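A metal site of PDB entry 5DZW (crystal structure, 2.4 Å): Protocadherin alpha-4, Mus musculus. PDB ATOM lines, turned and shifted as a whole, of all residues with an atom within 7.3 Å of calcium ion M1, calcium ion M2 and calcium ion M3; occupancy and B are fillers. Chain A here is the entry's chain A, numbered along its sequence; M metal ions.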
ATOM      1  N   GLU A 115       9.729 -29.889  -8.064  1.00  0.00           N
ATOM      2  CA  GLU A 115      10.605 -28.748  -8.338  1.00  0.00           C
ATOM      3  C   GLU A 115      10.195 -27.534  -7.501  1.00  0.00           C
ATOM      4  O   GLU A 115      10.992 -26.622  -7.285  1.00  0.00           O
ATOM      5  CB  GLU A 115      10.552 -28.405  -9.827  1.00  0.00           C
ATOM      6  CG  GLU A 115      11.522 -27.323 -10.271  1.00  0.00           C
ATOM      7  CD  GLU A 115      11.258 -26.844 -11.679  1.00  0.00           C
ATOM      8  OE1 GLU A 115      10.354 -27.397 -12.342  1.00  0.00           O
ATOM      9  OE2 GLU A 115      11.947 -25.902 -12.128  1.00  0.00           O
ATOM     10  N   LEU A 171      16.264 -26.181  -6.998  1.00  0.00           N
ATOM     11  CA  LEU A 171      16.234 -27.260  -7.984  1.00  0.00           C
ATOM     12  C   LEU A 171      15.423 -26.862  -9.215  1.00  0.00           C
ATOM     13  O   LEU A 171      14.369 -26.238  -9.103  1.00  0.00           O
ATOM     14  CB  LEU A 171      15.664 -28.536  -7.358  1.00  0.00           C
ATOM     15  CG  LEU A 171      14.168 -28.655  -7.051  1.00  0.00           C
ATOM     16  CD1 LEU A 171      13.816 -30.093  -6.713  1.00  0.00           C
ATOM     17  CD2 LEU A 171      13.734 -27.727  -5.912  1.00  0.00           C
ATOM     18  N   ASP A 172      15.922 -27.231 -10.387  1.00  0.00           N
ATOM     19  CA  ASP A 172      15.267 -26.906 -11.642  1.00  0.00           C
ATOM     20  C   ASP A 172      15.184 -28.128 -12.562  1.00  0.00           C
ATOM     21  O   ASP A 172      16.206 -28.671 -12.967  1.00  0.00           O
ATOM     22  CB  ASP A 172      15.998 -25.760 -12.349  1.00  0.00           C
ATOM     23  CG  ASP A 172      15.336 -25.362 -13.660  1.00  0.00           C
ATOM     24  OD1 ASP A 172      14.367 -24.570 -13.610  1.00  0.00           O
ATOM     25  OD2 ASP A 172      15.779 -25.832 -14.724  1.00  0.00           O
ATOM     26  N   ARG A 173      13.964 -28.525 -12.886  1.00  0.00           N
ATOM     27  CA  ARG A 173      13.710 -29.694 -13.713  1.00  0.00           C
ATOM     28  C   ARG A 173      14.331 -29.567 -15.113  1.00  0.00           C
ATOM     29  O   ARG A 173      14.868 -30.541 -15.643  1.00  0.00           O
ATOM     30  CB  ARG A 173      12.210 -29.949 -13.814  1.00  0.00           C
ATOM     31  CG  ARG A 173      11.788 -30.928 -14.892  1.00  0.00           C
ATOM     32  CD  ARG A 173      11.093 -30.208 -16.042  1.00  0.00           C
ATOM     33  NE  ARG A 173      10.456 -31.136 -16.968  1.00  0.00           N
ATOM     34  CZ  ARG A 173      11.054 -31.639 -18.046  1.00  0.00           C
ATOM     35  NH1 ARG A 173      10.403 -32.477 -18.841  1.00  0.00           N
ATOM     36  NH2 ARG A 173      12.302 -31.303 -18.329  1.00  0.00           N
ATOM     37  N   GLU A 174      14.250 -28.381 -15.692  1.00  0.00           N
ATOM     38  CA  GLU A 174      14.747 -28.148 -17.040  1.00  0.00           C
ATOM     39  C   GLU A 174      16.269 -28.239 -17.134  1.00  0.00           C
ATOM     40  O   GLU A 174      16.810 -28.724 -18.117  1.00  0.00           O
ATOM     41  CB  GLU A 174      14.276 -26.786 -17.570  1.00  0.00           C
ATOM     42  CG  GLU A 174      12.811 -26.733 -17.967  1.00  0.00           C
ATOM     43  CD  GLU A 174      11.870 -26.770 -16.778  1.00  0.00           C
ATOM     44  OE1 GLU A 174      12.317 -26.454 -15.656  1.00  0.00           O
ATOM     45  OE2 GLU A 174      10.684 -27.124 -16.968  1.00  0.00           O
ATOM     46  N   GLU A 175      16.943 -27.762 -16.090  1.00  0.00           N
ATOM     47  CA  GLU A 175      18.404 -27.804 -16.057  1.00  0.00           C
ATOM     48  C   GLU A 175      18.915 -29.234 -15.864  1.00  0.00           C
ATOM     49  O   GLU A 175      19.717 -29.729 -16.661  1.00  0.00           O
ATOM     50  CB  GLU A 175      18.938 -26.900 -14.943  1.00  0.00           C
ATOM     51  CG  GLU A 175      20.452 -26.876 -14.829  1.00  0.00           C
ATOM     52  CD  GLU A 175      20.954 -25.861 -13.826  1.00  0.00           C
ATOM     53  OE1 GLU A 175      20.223 -24.873 -13.572  1.00  0.00           O
ATOM     54  OE2 GLU A 175      22.063 -26.033 -13.292  1.00  0.00           O
ATOM     55  N   LEU A 204      10.193 -33.436 -10.460  1.00  0.00           N
ATOM     56  CA  LEU A 204       8.927 -33.285 -11.157  1.00  0.00           C
ATOM     57  C   LEU A 204       8.805 -31.900 -11.791  1.00  0.00           C
ATOM     58  O   LEU A 204       9.373 -30.928 -11.300  1.00  0.00           O
ATOM     59  CB  LEU A 204       7.761 -33.544 -10.201  1.00  0.00           C
ATOM     60  CG  LEU A 204       7.836 -34.855  -9.419  1.00  0.00           C
ATOM     61  CD1 LEU A 204       6.667 -35.004  -8.454  1.00  0.00           C
ATOM     62  CD2 LEU A 204       7.916 -36.050 -10.366  1.00  0.00           C
ATOM     63  N   ASP A 205       8.064 -31.824 -12.895  1.00  0.00           N
ATOM     64  CA  ASP A 205       7.930 -30.565 -13.633  1.00  0.00           C
ATOM     65  C   ASP A 205       6.944 -29.608 -12.964  1.00  0.00           C
ATOM     66  O   ASP A 205       5.759 -29.922 -12.822  1.00  0.00           O
ATOM     67  CB  ASP A 205       7.493 -30.843 -15.069  1.00  0.00           C
ATOM     68  CG  ASP A 205       7.361 -29.573 -15.895  1.00  0.00           C
ATOM     69  OD1 ASP A 205       8.170 -28.648 -15.697  1.00  0.00           O
ATOM     70  OD2 ASP A 205       6.447 -29.505 -16.742  1.00  0.00           O
ATOM     71  N   ALA A 206       7.442 -28.455 -12.552  1.00  0.00           N
ATOM     72  CA  ALA A 206       6.599 -27.406 -11.985  1.00  0.00           C
ATOM     73  C   ALA A 206       6.292 -26.358 -13.050  1.00  0.00           C
ATOM     74  O   ALA A 206       7.041 -26.212 -14.007  1.00  0.00           O
ATOM     75  CB  ALA A 206       7.264 -26.779 -10.781  1.00  0.00           C
ATOM     76  N   ASN A 207       5.204 -25.633 -12.865  1.00  0.00           N
ATOM     77  CA  ASN A 207       4.829 -24.580 -13.817  1.00  0.00           C
ATOM     78  C   ASN A 207       5.442 -23.239 -13.412  1.00  0.00           C
ATOM     79  O   ASN A 207       4.741 -22.320 -13.006  1.00  0.00           O
ATOM     80  CB  ASN A 207       3.309 -24.454 -13.912  1.00  0.00           C
ATOM     81  CG  ASN A 207       2.877 -23.589 -15.078  1.00  0.00           C
ATOM     82  OD1 ASN A 207       3.587 -23.459 -16.071  1.00  0.00           O
ATOM     83  ND2 ASN A 207       1.701 -22.971 -14.953  1.00  0.00           N
ATOM     84  N   ASP A 208       6.763 -23.148 -13.524  1.00  0.00           N
ATOM     85  CA  ASP A 208       7.483 -21.964 -13.077  1.00  0.00           C
ATOM     86  C   ASP A 208       8.187 -21.240 -14.225  1.00  0.00           C
ATOM     87  O   ASP A 208       9.028 -20.369 -14.000  1.00  0.00           O
ATOM     88  CB  ASP A 208       8.501 -22.336 -11.994  1.00  0.00           C
ATOM     89  CG  ASP A 208       9.464 -23.417 -12.445  1.00  0.00           C
ATOM     90  OD1 ASP A 208       9.046 -24.300 -13.222  1.00  0.00           O
ATOM     91  OD2 ASP A 208      10.638 -23.379 -12.012  1.00  0.00           O
ATOM     92  N   ASN A 209       7.842 -21.599 -15.461  1.00  0.00           N
ATOM     93  CA  ASN A 209       8.392 -20.933 -16.626  1.00  0.00           C
ATOM     94  C   ASN A 209       7.315 -20.414 -17.572  1.00  0.00           C
ATOM     95  O   ASN A 209       6.436 -21.168 -18.000  1.00  0.00           O
ATOM     96  CB  ASN A 209       9.337 -21.862 -17.388  1.00  0.00           C
ATOM     97  CG  ASN A 209      10.740 -21.885 -16.799  1.00  0.00           C
ATOM     98  OD1 ASN A 209      10.909 -21.756 -15.588  1.00  0.00           O
ATOM     99  ND2 ASN A 209      11.736 -22.036 -17.660  1.00  0.00           N
ATOM    100  N   ALA A 210       7.378 -19.124 -17.881  1.00  0.00           N
ATOM    101  CA  ALA A 210       6.415 -18.494 -18.782  1.00  0.00           C
ATOM    102  C   ALA A 210       6.830 -18.695 -20.240  1.00  0.00           C
ATOM    103  O   ALA A 210       8.018 -18.801 -20.545  1.00  0.00           O
ATOM    104  CB  ALA A 210       6.298 -17.012 -18.460  1.00  0.00           C
ATOM    105  N   PRO A 211       5.840 -18.752 -21.152  1.00  0.00           N
ATOM    106  CA  PRO A 211       6.125 -18.867 -22.576  1.00  0.00           C
ATOM    107  C   PRO A 211       6.869 -17.655 -23.124  1.00  0.00           C
ATOM    108  O   PRO A 211       6.705 -16.551 -22.598  1.00  0.00           O
ATOM    109  CB  PRO A 211       4.731 -18.986 -23.205  1.00  0.00           C
ATOM    110  CG  PRO A 211       3.794 -18.434 -22.192  1.00  0.00           C
ATOM    111  CD  PRO A 211       4.398 -18.781 -20.865  1.00  0.00           C
ATOM    112  N   ASP A 239       7.973 -22.708 -24.682  1.00  0.00           N
ATOM    113  CA  ASP A 239       7.933 -22.815 -23.231  1.00  0.00           C
ATOM    114  C   ASP A 239       8.684 -24.059 -22.758  1.00  0.00           C
ATOM    115  O   ASP A 239       8.539 -25.136 -23.334  1.00  0.00           O
ATOM    116  CB  ASP A 239       6.481 -22.834 -22.737  1.00  0.00           C
ATOM    117  CG  ASP A 239       6.370 -22.718 -21.229  1.00  0.00           C
ATOM    118  OD1 ASP A 239       7.380 -22.350 -20.579  1.00  0.00           O
ATOM    119  OD2 ASP A 239       5.280 -22.985 -20.696  1.00  0.00           O
ATOM    120  N   LEU A 240       9.476 -23.896 -21.697  1.00  0.00           N
ATOM    121  CA  LEU A 240      10.373 -24.953 -21.251  1.00  0.00           C
ATOM    122  C   LEU A 240       9.669 -26.064 -20.473  1.00  0.00           C
ATOM    123  O   LEU A 240      10.169 -27.180 -20.395  1.00  0.00           O
ATOM    124  CB  LEU A 240      11.493 -24.354 -20.397  1.00  0.00           C
ATOM    125  CG  LEU A 240      12.472 -23.457 -21.145  1.00  0.00           C
ATOM    126  CD1 LEU A 240      13.589 -22.982 -20.229  1.00  0.00           C
ATOM    127  CD2 LEU A 240      13.050 -24.187 -22.354  1.00  0.00           C
ATOM    128  N   ASP A 241       8.505 -25.759 -19.911  1.00  0.00           N
ATOM    129  CA  ASP A 241       7.752 -26.761 -19.161  1.00  0.00           C
ATOM    130  C   ASP A 241       7.107 -27.782 -20.090  1.00  0.00           C
ATOM    131  O   ASP A 241       7.022 -27.563 -21.303  1.00  0.00           O
ATOM    132  CB  ASP A 241       6.691 -26.092 -18.281  1.00  0.00           C
ATOM    133  CG  ASP A 241       7.285 -25.140 -17.270  1.00  0.00           C
ATOM    134  OD1 ASP A 241       8.527 -25.060 -17.184  1.00  0.00           O
ATOM    135  OD2 ASP A 241       6.515 -24.482 -16.544  1.00  0.00           O
ATOM    136  N   GLU A 242       6.659 -28.894 -19.522  1.00  0.00           N
ATOM    137  CA  GLU A 242       6.084 -29.980 -20.316  1.00  0.00           C
ATOM    138  C   GLU A 242       4.619 -30.232 -19.959  1.00  0.00           C
ATOM    139  O   GLU A 242       4.120 -29.731 -18.954  1.00  0.00           O
ATOM    140  CB  GLU A 242       6.897 -31.260 -20.125  1.00  0.00           C
ATOM    141  N   VAL A 244       0.608 -29.967 -20.038  1.00  0.00           N
ATOM    142  CA  VAL A 244      -0.297 -28.842 -20.168  1.00  0.00           C
ATOM    143  C   VAL A 244       0.391 -27.548 -19.736  1.00  0.00           C
ATOM    144  O   VAL A 244      -0.053 -26.453 -20.066  1.00  0.00           O
ATOM    145  CB  VAL A 244      -1.582 -29.038 -19.340  1.00  0.00           C
ATOM    146  CG1 VAL A 244      -2.385 -30.215 -19.865  1.00  0.00           C
ATOM    147  CG2 VAL A 244      -1.251 -29.228 -17.862  1.00  0.00           C
ATOM    148  N   ASN A 245       1.488 -27.687 -18.986  1.00  0.00           N
ATOM    149  CA  ASN A 245       2.277 -26.541 -18.574  1.00  0.00           C
ATOM    150  C   ASN A 245       3.157 -26.036 -19.709  1.00  0.00           C
ATOM    151  O   ASN A 245       3.773 -24.980 -19.604  1.00  0.00           O
ATOM    152  CB  ASN A 245       3.139 -26.889 -17.359  1.00  0.00           C
ATOM    153  CG  ASN A 245       2.308 -27.275 -16.145  1.00  0.00           C
ATOM    154  OD1 ASN A 245       1.089 -27.358 -16.224  1.00  0.00           O
ATOM    155  ND2 ASN A 245       2.980 -27.514 -15.033  1.00  0.00           N
ATOM    156  N   GLY A 246       3.194 -26.800 -20.794  1.00  0.00           N
ATOM    157  CA  GLY A 246       3.999 -26.448 -21.952  1.00  0.00           C
ATOM    158  C   GLY A 246       3.178 -25.956 -23.133  1.00  0.00           C
ATOM    159  O   GLY A 246       3.638 -25.134 -23.925  1.00  0.00           O
ATOM    160  N   ASP A 247       1.950 -26.471 -23.262  1.00  0.00           N
ATOM    161  CA  ASP A 247       1.068 -26.077 -24.359  1.00  0.00           C
ATOM    162  C   ASP A 247       0.629 -24.626 -24.224  1.00  0.00           C
ATOM    163  O   ASP A 247       0.245 -24.187 -23.143  1.00  0.00           O
ATOM    164  CB  ASP A 247      -0.152 -26.999 -24.419  1.00  0.00           C
ATOM    165  CG  ASP A 247       0.184 -28.387 -24.924  1.00  0.00           C
ATOM    166  OD1 ASP A 247       1.293 -28.881 -24.627  1.00  0.00           O
ATOM    167  OD2 ASP A 247      -0.658 -28.990 -25.616  1.00  0.00           O
ATOM    168  N   ILE A 248       0.688 -23.885 -25.335  1.00  0.00           N
ATOM    169  CA  ILE A 248       0.410 -22.454 -25.314  1.00  0.00           C
ATOM    170  C   ILE A 248      -0.812 -22.074 -26.148  1.00  0.00           C
ATOM    171  O   ILE A 248      -0.945 -22.483 -27.299  1.00  0.00           O
ATOM    172  CB  ILE A 248       1.624 -21.657 -25.834  1.00  0.00           C
ATOM    173  CG1 ILE A 248       2.913 -22.125 -25.151  1.00  0.00           C
ATOM    174  CG2 ILE A 248       1.417 -20.159 -25.621  1.00  0.00           C
ATOM    175  CD1 ILE A 248       4.165 -21.513 -25.727  1.00  0.00           C
ATOM    176  N   ASP A 295      -0.016 -20.392 -21.085  1.00  0.00           N
ATOM    177  CA  ASP A 295       0.028 -21.848 -20.981  1.00  0.00           C
ATOM    178  C   ASP A 295      -1.230 -22.394 -20.326  1.00  0.00           C
ATOM    179  O   ASP A 295      -2.122 -21.640 -19.935  1.00  0.00           O
ATOM    180  CB  ASP A 295       1.280 -22.305 -20.212  1.00  0.00           C
ATOM    181  CG  ASP A 295       1.526 -21.493 -18.959  1.00  0.00           C
ATOM    182  OD1 ASP A 295       0.545 -21.079 -18.307  1.00  0.00           O
ATOM    183  OD2 ASP A 295       2.702 -21.269 -18.613  1.00  0.00           O
ATOM    184  N   LYS A 296      -1.316 -23.717 -20.199  1.00  0.00           N
ATOM    185  CA  LYS A 296      -2.522 -24.366 -19.693  1.00  0.00           C
ATOM    186  C   LYS A 296      -2.284 -25.088 -18.374  1.00  0.00           C
ATOM    187  O   LYS A 296      -2.780 -26.196 -18.170  1.00  0.00           O
ATOM    188  CB  LYS A 296      -3.061 -25.348 -20.741  1.00  0.00           C
ATOM    189  CG  LYS A 296      -3.319 -24.735 -22.106  1.00  0.00           C
ATOM    190  CD  LYS A 296      -3.793 -25.783 -23.103  1.00  0.00           C
ATOM    191  N   GLY A 297      -1.530 -24.461 -17.477  1.00  0.00           N
ATOM    192  CA  GLY A 297      -1.256 -25.038 -16.178  1.00  0.00           C
ATOM    193  C   GLY A 297      -2.298 -24.652 -15.154  1.00  0.00           C
ATOM    194  O   GLY A 297      -3.227 -23.896 -15.452  1.00  0.00           O
ATOM    195  N   LEU A 299      -1.744 -22.857 -12.382  1.00  0.00           N
ATOM    196  CA  LEU A 299      -1.492 -21.429 -12.268  1.00  0.00           C
ATOM    197  C   LEU A 299      -0.845 -20.946 -13.553  1.00  0.00           C
ATOM    198  O   LEU A 299       0.376 -21.055 -13.715  1.00  0.00           O
ATOM    199  CB  LEU A 299      -0.610 -21.112 -11.061  1.00  0.00           C
ATOM    200  CG  LEU A 299      -0.305 -19.633 -10.837  1.00  0.00           C
ATOM    201  CD1 LEU A 299      -1.593 -18.829 -10.753  1.00  0.00           C
ATOM    202  CD2 LEU A 299       0.546 -19.434  -9.598  1.00  0.00           C
ATOM    203  N   PRO A 300      -1.656 -20.422 -14.483  1.00  0.00           N
ATOM    204  CA  PRO A 300      -1.203 -20.028 -15.822  1.00  0.00           C
ATOM    205  C   PRO A 300      -0.161 -18.923 -15.810  1.00  0.00           C
ATOM    206  O   PRO A 300      -0.277 -17.967 -15.029  1.00  0.00           O
ATOM    207  CB  PRO A 300      -2.489 -19.550 -16.496  1.00  0.00           C
ATOM    208  CG  PRO A 300      -3.601 -20.178 -15.721  1.00  0.00           C
ATOM    209  CD  PRO A 300      -3.108 -20.225 -14.312  1.00  0.00           C
ATOM    210  N   LEU A 301       0.845 -19.051 -16.666  1.00  0.00           N
ATOM    211  CA  LEU A 301       1.823 -17.988 -16.878  1.00  0.00           C
ATOM    212  C   LEU A 301       1.668 -17.421 -18.289  1.00  0.00           C
ATOM    213  O   LEU A 301       1.361 -18.154 -19.234  1.00  0.00           O
ATOM    214  CB  LEU A 301       3.244 -18.509 -16.671  1.00  0.00           C
ATOM    215  CG  LEU A 301       3.618 -18.880 -15.233  1.00  0.00           C
ATOM    216  CD1 LEU A 301       5.090 -19.247 -15.138  1.00  0.00           C
ATOM    217  CD2 LEU A 301       3.280 -17.741 -14.283  1.00  0.00           C
HETATM  218 CA    CA M   1       4.855 -22.996 -18.368  1.00  0.00          CA
HETATM  219 CA    CA M   2       9.149 -26.474 -15.056  1.00  0.00          CA
HETATM  220 CA    CA M   3      11.383 -24.741 -14.201  1.00  0.00          CA
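The backbone NH of Arg 173 sits close to the side-chain carboxylate of Glu 115 (3.4 Å). The backbone NH of Ala 206 lies within hydrogen-bond range of the side-chain carboxylate of Glu 115, 3.1 Å away. O of Leu 299 lies within hydrogen-bond range of ND2 of Asn 207. The side-chain carboxylate (OD2) of Asp 172 is in hydrogen-bond range of the backbone NH (N) of Glu 175 (2.6 Å). N of Glu 115 lies close to O of Leu 204, at 3.4 Å. The side-chain carboxylate (OD2) of Asp 172 is in hydrogen-bond range of the backbone NH (N) of Glu 174. OD2 of Asp 205 is in hydrogen-bond range of N of Glu 242 (2.9 Å). OD1 of Asp 295 lies within hydrogen-bond range of N of Leu 301.
Five residues have an atom within 4 Å of calcium ion M3: Glu 115, Asp 172, Glu 174, Asp 208 and Asn 209. Along chain A the residues within 4 Å of calcium ion M3 span positions 115 to 209. The nearest printed residue that does not touch calcium ion M3 is Asp 241 (4.1 Å).
Calcium ion M3 is bound by OE1 of Glu 174 (2.4 Å), OE2 of Glu 115 (2.4 Å), OD1 of Asp 208 (2.6 Å) and OD2 of Asp 208 (2.7 Å). Slightly farther from calcium ion M3 lies the side-chain carboxylate (OD1) of Asp 172 (3.0 Å).
Of the 29 residues printed, 6 come within 4 Å of calcium ion M1. The nearest printed residue that does not touch calcium ion M1 is Ala 210 (4.6 Å).
Calcium ion M2 is bound by the backbone carbonyl oxygen (O) of Ala 206. The side-chain carboxylate (OD1) of Asp 205 binds calcium ion M2, at 2.5 Å. OE2 of Glu 174 binds calcium ion M2 (2.5 Å). OD1 of Asp 241 is bound to calcium ion M2. OD1 of Asp 208 is bound to calcium ion M2 (2.8 Å). Calcium ion M2 has five donor atoms within binding distance. Slightly farther from calcium ion M2 lies the side-chain carboxylate (OE1) of Glu 115 (3.1 Å).
Calcium ion M1 is bound by the side-chain carboxylate of Asp 239 (2.4 Å), the backbone carbonyl oxygen of Asn 209 (2.4 Å), the backbone carbonyl oxygen of Asn 245 (2.6 Å), the side-chain amide oxygen of Asn 207 (2.7 Å), the side-chain carboxylate of Asp 295 (2.8 Å) and the side-chain carboxylate of Asp 241 (2.9 Å).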
